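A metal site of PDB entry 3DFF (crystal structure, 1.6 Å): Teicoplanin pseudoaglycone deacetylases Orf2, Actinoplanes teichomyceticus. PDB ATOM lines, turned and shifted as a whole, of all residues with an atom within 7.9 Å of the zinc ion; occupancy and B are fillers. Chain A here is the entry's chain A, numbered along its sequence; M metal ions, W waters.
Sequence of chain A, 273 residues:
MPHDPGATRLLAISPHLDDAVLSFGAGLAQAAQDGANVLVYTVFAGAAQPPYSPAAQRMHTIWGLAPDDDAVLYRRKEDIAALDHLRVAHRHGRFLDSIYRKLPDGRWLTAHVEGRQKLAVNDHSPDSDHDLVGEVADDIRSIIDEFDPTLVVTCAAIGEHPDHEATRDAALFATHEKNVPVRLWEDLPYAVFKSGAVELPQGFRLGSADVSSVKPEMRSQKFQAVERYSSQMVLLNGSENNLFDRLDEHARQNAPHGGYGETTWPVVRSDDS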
ATOM      1  N   SER A  14      22.384  -4.670   5.727  1.00  0.00           N
ATOM      2  CA  SER A  14      21.119  -5.281   6.116  1.00  0.00           C
ATOM      3  C   SER A  14      21.190  -6.807   5.946  1.00  0.00           C
ATOM      4  O   SER A  14      21.640  -7.277   4.912  1.00  0.00           O
ATOM      5  CB  SER A  14      20.015  -4.715   5.229  1.00  0.00           C
ATOM      6  OG  SER A  14      18.743  -5.138   5.689  1.00  0.00           O
ATOM      7  N   PRO A  15      20.715  -7.583   6.937  1.00  0.00           N
ATOM      8  CA  PRO A  15      20.659  -9.037   6.735  1.00  0.00           C
ATOM      9  C   PRO A  15      19.725  -9.382   5.584  1.00  0.00           C
ATOM     10  O   PRO A  15      20.143 -10.094   4.653  1.00  0.00           O
ATOM     11  CB  PRO A  15      20.124  -9.596   8.072  1.00  0.00           C
ATOM     12  CG  PRO A  15      20.155  -8.482   9.008  1.00  0.00           C
ATOM     13  CD  PRO A  15      20.202  -7.176   8.261  1.00  0.00           C
ATOM     14  N   HIS A  16      18.485  -8.906   5.640  1.00  0.00           N
ATOM     15  CA  HIS A  16      17.458  -9.252   4.658  1.00  0.00           C
ATOM     16  C   HIS A  16      16.935  -8.025   3.962  1.00  0.00           C
ATOM     17  O   HIS A  16      17.200  -6.895   4.377  1.00  0.00           O
ATOM     18  CB  HIS A  16      16.267  -9.935   5.328  1.00  0.00           C
ATOM     19  CG  HIS A  16      16.624 -11.185   6.059  1.00  0.00           C
ATOM     20  ND1 HIS A  16      16.412 -11.331   7.410  1.00  0.00           N
ATOM     21  CD2 HIS A  16      17.156 -12.351   5.618  1.00  0.00           C
ATOM     22  CE1 HIS A  16      16.799 -12.549   7.779  1.00  0.00           C
ATOM     23  NE2 HIS A  16      17.279 -13.168   6.707  1.00  0.00           N
ATOM     24  N   LEU A  17      16.160  -8.261   2.901  1.00  0.00           N
ATOM     25  CA  LEU A  17      15.545  -7.202   2.122  1.00  0.00           C
ATOM     26  C   LEU A  17      14.329  -6.629   2.858  1.00  0.00           C
ATOM     27  O   LEU A  17      13.180  -7.034   2.604  1.00  0.00           O
ATOM     28  CB  LEU A  17      15.193  -7.734   0.722  1.00  0.00           C
ATOM     29  CG  LEU A  17      16.393  -8.230  -0.098  1.00  0.00           C
ATOM     30  CD1 LEU A  17      15.968  -9.183  -1.187  1.00  0.00           C
ATOM     31  CD2 LEU A  17      17.148  -7.026  -0.731  1.00  0.00           C
ATOM     32  N   ASP A  18      14.616  -5.714   3.784  1.00  0.00           N
ATOM     33  CA  ASP A  18      13.622  -4.991   4.598  1.00  0.00           C
ATOM     34  C   ASP A  18      14.215  -4.471   5.904  1.00  0.00           C
ATOM     35  O   ASP A  18      13.741  -3.482   6.443  1.00  0.00           O
ATOM     36  CB  ASP A  18      12.352  -5.794   4.899  1.00  0.00           C
ATOM     37  CG  ASP A  18      12.630  -7.139   5.619  1.00  0.00           C
ATOM     38  OD1 ASP A  18      13.779  -7.458   5.989  1.00  0.00           O
ATOM     39  OD2 ASP A  18      11.652  -7.906   5.775  1.00  0.00           O
ATOM     40  N   ASP A  19      15.246  -5.128   6.427  1.00  0.00           N
ATOM     41  CA  ASP A  19      15.641  -4.876   7.826  1.00  0.00           C
ATOM     42  C   ASP A  19      16.177  -3.463   8.032  1.00  0.00           C
ATOM     43  O   ASP A  19      15.838  -2.813   9.018  1.00  0.00           O
ATOM     44  CB  ASP A  19      16.689  -5.896   8.308  1.00  0.00           C
ATOM     45  CG  ASP A  19      16.111  -7.285   8.501  1.00  0.00           C
ATOM     46  OD1 ASP A  19      15.136  -7.448   9.258  1.00  0.00           O
ATOM     47  OD2 ASP A  19      16.637  -8.225   7.875  1.00  0.00           O
ATOM     48  N   ALA A  20      17.011  -3.000   7.106  1.00  0.00           N
ATOM     49  CA  ALA A  20      17.615  -1.661   7.233  1.00  0.00           C
ATOM     50  C   ALA A  20      16.544  -0.592   7.202  1.00  0.00           C
ATOM     51  O   ALA A  20      16.630   0.401   7.970  1.00  0.00           O
ATOM     52  CB  ALA A  20      18.641  -1.431   6.100  1.00  0.00           C
ATOM     53  N   LEU A  22      13.192  -0.968   7.888  1.00  0.00           N
ATOM     54  CA  LEU A  22      12.404  -1.103   9.121  1.00  0.00           C
ATOM     55  C   LEU A  22      13.100  -0.533  10.333  1.00  0.00           C
ATOM     56  O   LEU A  22      12.458   0.108  11.194  1.00  0.00           O
ATOM     57  CB  LEU A  22      12.136  -2.576   9.403  1.00  0.00           C
ATOM     58  CG  LEU A  22      11.047  -3.236   8.563  1.00  0.00           C
ATOM     59  CD1 LEU A  22      11.181  -4.745   8.662  1.00  0.00           C
ATOM     60  CD2 LEU A  22       9.651  -2.762   9.001  1.00  0.00           C
ATOM     61  N   SER A  23      14.405  -0.772  10.426  1.00  0.00           N
ATOM     62  CA  SER A  23      15.141  -0.449  11.652  1.00  0.00           C
ATOM     63  C   SER A  23      15.789   0.915  11.636  1.00  0.00           C
ATOM     64  O   SER A  23      15.982   1.519  12.707  1.00  0.00           O
ATOM     65  CB  SER A  23      16.211  -1.507  11.940  1.00  0.00           C
ATOM     66  OG  SER A  23      15.641  -2.803  12.022  1.00  0.00           O
ATOM     67  N   PHE A  44      21.807 -11.148   2.530  1.00  0.00           N
ATOM     68  CA  PHE A  44      21.066 -12.345   2.134  1.00  0.00           C
ATOM     69  C   PHE A  44      20.053 -12.039   1.034  1.00  0.00           C
ATOM     70  O   PHE A  44      18.855 -12.299   1.160  1.00  0.00           O
ATOM     71  CB  PHE A  44      20.472 -13.044   3.378  1.00  0.00           C
ATOM     72  CG  PHE A  44      21.523 -13.603   4.267  1.00  0.00           C
ATOM     73  CD1 PHE A  44      22.158 -14.815   3.952  1.00  0.00           C
ATOM     74  CD2 PHE A  44      21.961 -12.892   5.394  1.00  0.00           C
ATOM     75  CE1 PHE A  44      23.194 -15.342   4.762  1.00  0.00           C
ATOM     76  CE2 PHE A  44      22.998 -13.414   6.212  1.00  0.00           C
ATOM     77  CZ  PHE A  44      23.620 -14.644   5.875  1.00  0.00           C
ATOM     78  N   ARG A  75      11.437  -9.519  -4.067  1.00  0.00           N
ATOM     79  CA  ARG A  75      11.902  -8.811  -2.881  1.00  0.00           C
ATOM     80  C   ARG A  75      13.001  -7.799  -3.203  1.00  0.00           C
ATOM     81  O   ARG A  75      13.100  -6.733  -2.581  1.00  0.00           O
ATOM     82  CB  ARG A  75      12.348  -9.809  -1.810  1.00  0.00           C
ATOM     83  CG  ARG A  75      11.185 -10.604  -1.238  1.00  0.00           C
ATOM     84  CD  ARG A  75      11.610 -11.361   0.015  1.00  0.00           C
ATOM     85  NE  ARG A  75      11.903 -10.453   1.126  1.00  0.00           N
ATOM     86  CZ  ARG A  75      12.414 -10.842   2.295  1.00  0.00           C
ATOM     87  NH1 ARG A  75      12.705 -12.118   2.486  1.00  0.00           N
ATOM     88  NH2 ARG A  75      12.652  -9.962   3.251  1.00  0.00           N
ATOM     89  N   ASP A  97      19.224 -16.576   1.682  1.00  0.00           N
ATOM     90  CA  ASP A  97      18.407 -16.546   2.883  1.00  0.00           C
ATOM     91  C   ASP A  97      18.360 -17.943   3.521  1.00  0.00           C
ATOM     92  O   ASP A  97      18.364 -18.939   2.816  1.00  0.00           O
ATOM     93  CB  ASP A  97      16.994 -16.109   2.553  1.00  0.00           C
ATOM     94  CG  ASP A  97      16.175 -15.881   3.816  1.00  0.00           C
ATOM     95  OD1 ASP A  97      15.802 -16.867   4.511  1.00  0.00           O
ATOM     96  OD2 ASP A  97      15.943 -14.730   4.145  1.00  0.00           O
ATOM     97  N   CYS A 155      22.882  -4.648  11.996  1.00  0.00           N
ATOM     98  CA  CYS A 155      21.860  -5.000  12.968  1.00  0.00           C
ATOM     99  C   CYS A 155      22.451  -5.508  14.277  1.00  0.00           C
ATOM    100  O   CYS A 155      23.511  -6.144  14.301  1.00  0.00           O
ATOM    101  CB  CYS A 155      20.937  -6.076  12.394  1.00  0.00           C
ATOM    102  SG  CYS A 155      21.807  -7.597  11.904  1.00  0.00           S
ATOM    103  N   HIS A 161      17.718 -14.058  14.945  1.00  0.00           N
ATOM    104  CA  HIS A 161      17.591 -14.714  13.635  1.00  0.00           C
ATOM    105  C   HIS A 161      19.009 -15.062  13.172  1.00  0.00           C
ATOM    106  O   HIS A 161      19.914 -14.197  13.177  1.00  0.00           O
ATOM    107  CB  HIS A 161      16.909 -13.833  12.585  1.00  0.00           C
ATOM    108  CG  HIS A 161      16.657 -14.537  11.286  1.00  0.00           C
ATOM    109  ND1 HIS A 161      15.395 -14.795  10.817  1.00  0.00           N
ATOM    110  CD2 HIS A 161      17.523 -15.048  10.372  1.00  0.00           C
ATOM    111  CE1 HIS A 161      15.480 -15.431   9.660  1.00  0.00           C
ATOM    112  NE2 HIS A 161      16.763 -15.605   9.376  1.00  0.00           N
ATOM    113  N   ASP A 163      20.464 -15.379  10.396  1.00  0.00           N
ATOM    114  CA  ASP A 163      20.971 -14.537   9.334  1.00  0.00           C
ATOM    115  C   ASP A 163      21.361 -13.173   9.879  1.00  0.00           C
ATOM    116  O   ASP A 163      22.296 -12.526   9.374  1.00  0.00           O
ATOM    117  CB  ASP A 163      19.916 -14.345   8.230  1.00  0.00           C
ATOM    118  CG  ASP A 163      19.682 -15.616   7.411  1.00  0.00           C
ATOM    119  OD1 ASP A 163      20.518 -16.537   7.456  1.00  0.00           O
ATOM    120  OD2 ASP A 163      18.668 -15.661   6.674  1.00  0.00           O
ATOM    121  N   HIS A 164      20.632 -12.704  10.888  1.00  0.00           N
ATOM    122  CA  HIS A 164      20.957 -11.423  11.533  1.00  0.00           C
ATOM    123  C   HIS A 164      22.237 -11.543  12.333  1.00  0.00           C
ATOM    124  O   HIS A 164      23.091 -10.642  12.284  1.00  0.00           O
ATOM    125  CB  HIS A 164      19.820 -10.965  12.455  1.00  0.00           C
ATOM    126  CG  HIS A 164      18.648 -10.406  11.713  1.00  0.00           C
ATOM    127  ND1 HIS A 164      17.979  -9.266  12.128  1.00  0.00           N
ATOM    128  CD2 HIS A 164      18.025 -10.817  10.580  1.00  0.00           C
ATOM    129  CE1 HIS A 164      17.004  -9.000  11.278  1.00  0.00           C
ATOM    130  NE2 HIS A 164      17.007  -9.929  10.325  1.00  0.00           N
ATOM    131  N   ASP A 187      16.987  -3.921  16.108  1.00  0.00           N
ATOM    132  CA  ASP A 187      16.202  -4.620  15.076  1.00  0.00           C
ATOM    133  C   ASP A 187      14.712  -4.370  15.300  1.00  0.00           C
ATOM    134  O   ASP A 187      14.211  -4.673  16.380  1.00  0.00           O
ATOM    135  CB  ASP A 187      16.443  -6.150  15.080  1.00  0.00           C
ATOM    136  CG  ASP A 187      17.907  -6.514  15.043  1.00  0.00           C
ATOM    137  OD1 ASP A 187      18.291  -7.213  14.072  1.00  0.00           O
ATOM    138  OD2 ASP A 187      18.654  -6.134  15.976  1.00  0.00           O
ATOM    139  N   LEU A 188      14.053  -3.820  14.297  1.00  0.00           N
ATOM    140  CA  LEU A 188      12.590  -3.650  14.317  1.00  0.00           C
ATOM    141  C   LEU A 188      11.900  -4.491  13.259  1.00  0.00           C
ATOM    142  O   LEU A 188      12.432  -4.662  12.149  1.00  0.00           O
ATOM    143  CB  LEU A 188      12.204  -2.173  14.149  1.00  0.00           C
ATOM    144  CG  LEU A 188      12.794  -1.216  15.192  1.00  0.00           C
ATOM    145  CD1 LEU A 188      12.464   0.212  14.833  1.00  0.00           C
ATOM    146  CD2 LEU A 188      12.226  -1.536  16.580  1.00  0.00           C
ATOM    147  N   TYR A 190      11.348  -6.559  15.773  1.00  0.00           N
ATOM    148  CA  TYR A 190      11.777  -7.581  16.755  1.00  0.00           C
ATOM    149  C   TYR A 190      11.873  -7.051  18.176  1.00  0.00           C
ATOM    150  O   TYR A 190      11.506  -7.725  19.134  1.00  0.00           O
ATOM    151  CB  TYR A 190      13.178  -8.096  16.428  1.00  0.00           C
ATOM    152  CG  TYR A 190      13.294  -9.085  15.295  1.00  0.00           C
ATOM    153  CD1 TYR A 190      12.990 -10.431  15.486  1.00  0.00           C
ATOM    154  CD2 TYR A 190      13.764  -8.679  14.043  1.00  0.00           C
ATOM    155  CE1 TYR A 190      13.132 -11.355  14.464  1.00  0.00           C
ATOM    156  CE2 TYR A 190      13.921  -9.597  13.003  1.00  0.00           C
ATOM    157  CZ  TYR A 190      13.611 -10.929  13.221  1.00  0.00           C
ATOM    158  OH  TYR A 190      13.761 -11.832  12.208  1.00  0.00           O
ATOM    159  N   GLN A 232       5.958  -8.225   2.739  1.00  0.00           N
ATOM    160  CA  GLN A 232       6.155  -8.329   4.167  1.00  0.00           C
ATOM    161  C   GLN A 232       5.046  -7.698   4.996  1.00  0.00           C
ATOM    162  O   GLN A 232       5.005  -7.889   6.198  1.00  0.00           O
ATOM    163  CB  GLN A 232       7.489  -7.687   4.543  1.00  0.00           C
ATOM    164  CG  GLN A 232       8.665  -8.231   3.758  1.00  0.00           C
ATOM    165  CD  GLN A 232       8.841  -9.732   3.906  1.00  0.00           C
ATOM    166  OE1 GLN A 232       8.957 -10.249   5.027  1.00  0.00           O
ATOM    167  NE2 GLN A 232       8.893 -10.436   2.775  1.00  0.00           N
HETATM  168 ZN    ZN M   1      15.613  -9.900   8.708  1.00  0.00          ZN
HETATM  169  O   HOH W   1      14.477 -11.127   9.813  1.00  0.00           O
HETATM  170  O   HOH W   2      13.956  -9.534   7.467  1.00  0.00           O
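A ring nitrogen (NE2) of His 16 sits at hydrogen-bond distance from the side-chain carboxylate (OD2) of Asp 163. O of His 16 sits at hydrogen-bond distance from OG of Ser 14. OD2 of Asp 97 sits close to NE2 of His 16, at 3.3 Å. The backbone carbonyl oxygen (O) of Asp 19 is in hydrogen-bond range of the side-chain hydroxyl (OG) of Ser 23, at 3.0 Å. A ring nitrogen (ND1) of His 164 lies within hydrogen-bond range of the side-chain carboxylate (OD1) of Asp 187 (2.8 Å). The backbone carbonyl oxygen (O) of His 164 lies within hydrogen-bond range of the side-chain sulfur (SG) of Cys 155 (3.3 Å).
Three residues have an atom within 4 Å of the zinc ion: His 16, Asp 19 and His 164.
The zinc ion is bound by water W1 (2.0 Å), a ring nitrogen (ND1) of His 16 (2.1 Å), water W2 (2.1 Å), the side-chain carboxylate (OD2) of Asp 19 (2.1 Å), a ring nitrogen (NE2) of His 164 (2.1 Å) and the side-chain carboxylate (OD1) of Asp 19 (2.6 Å). The zinc ion has six donor atoms within binding distance.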
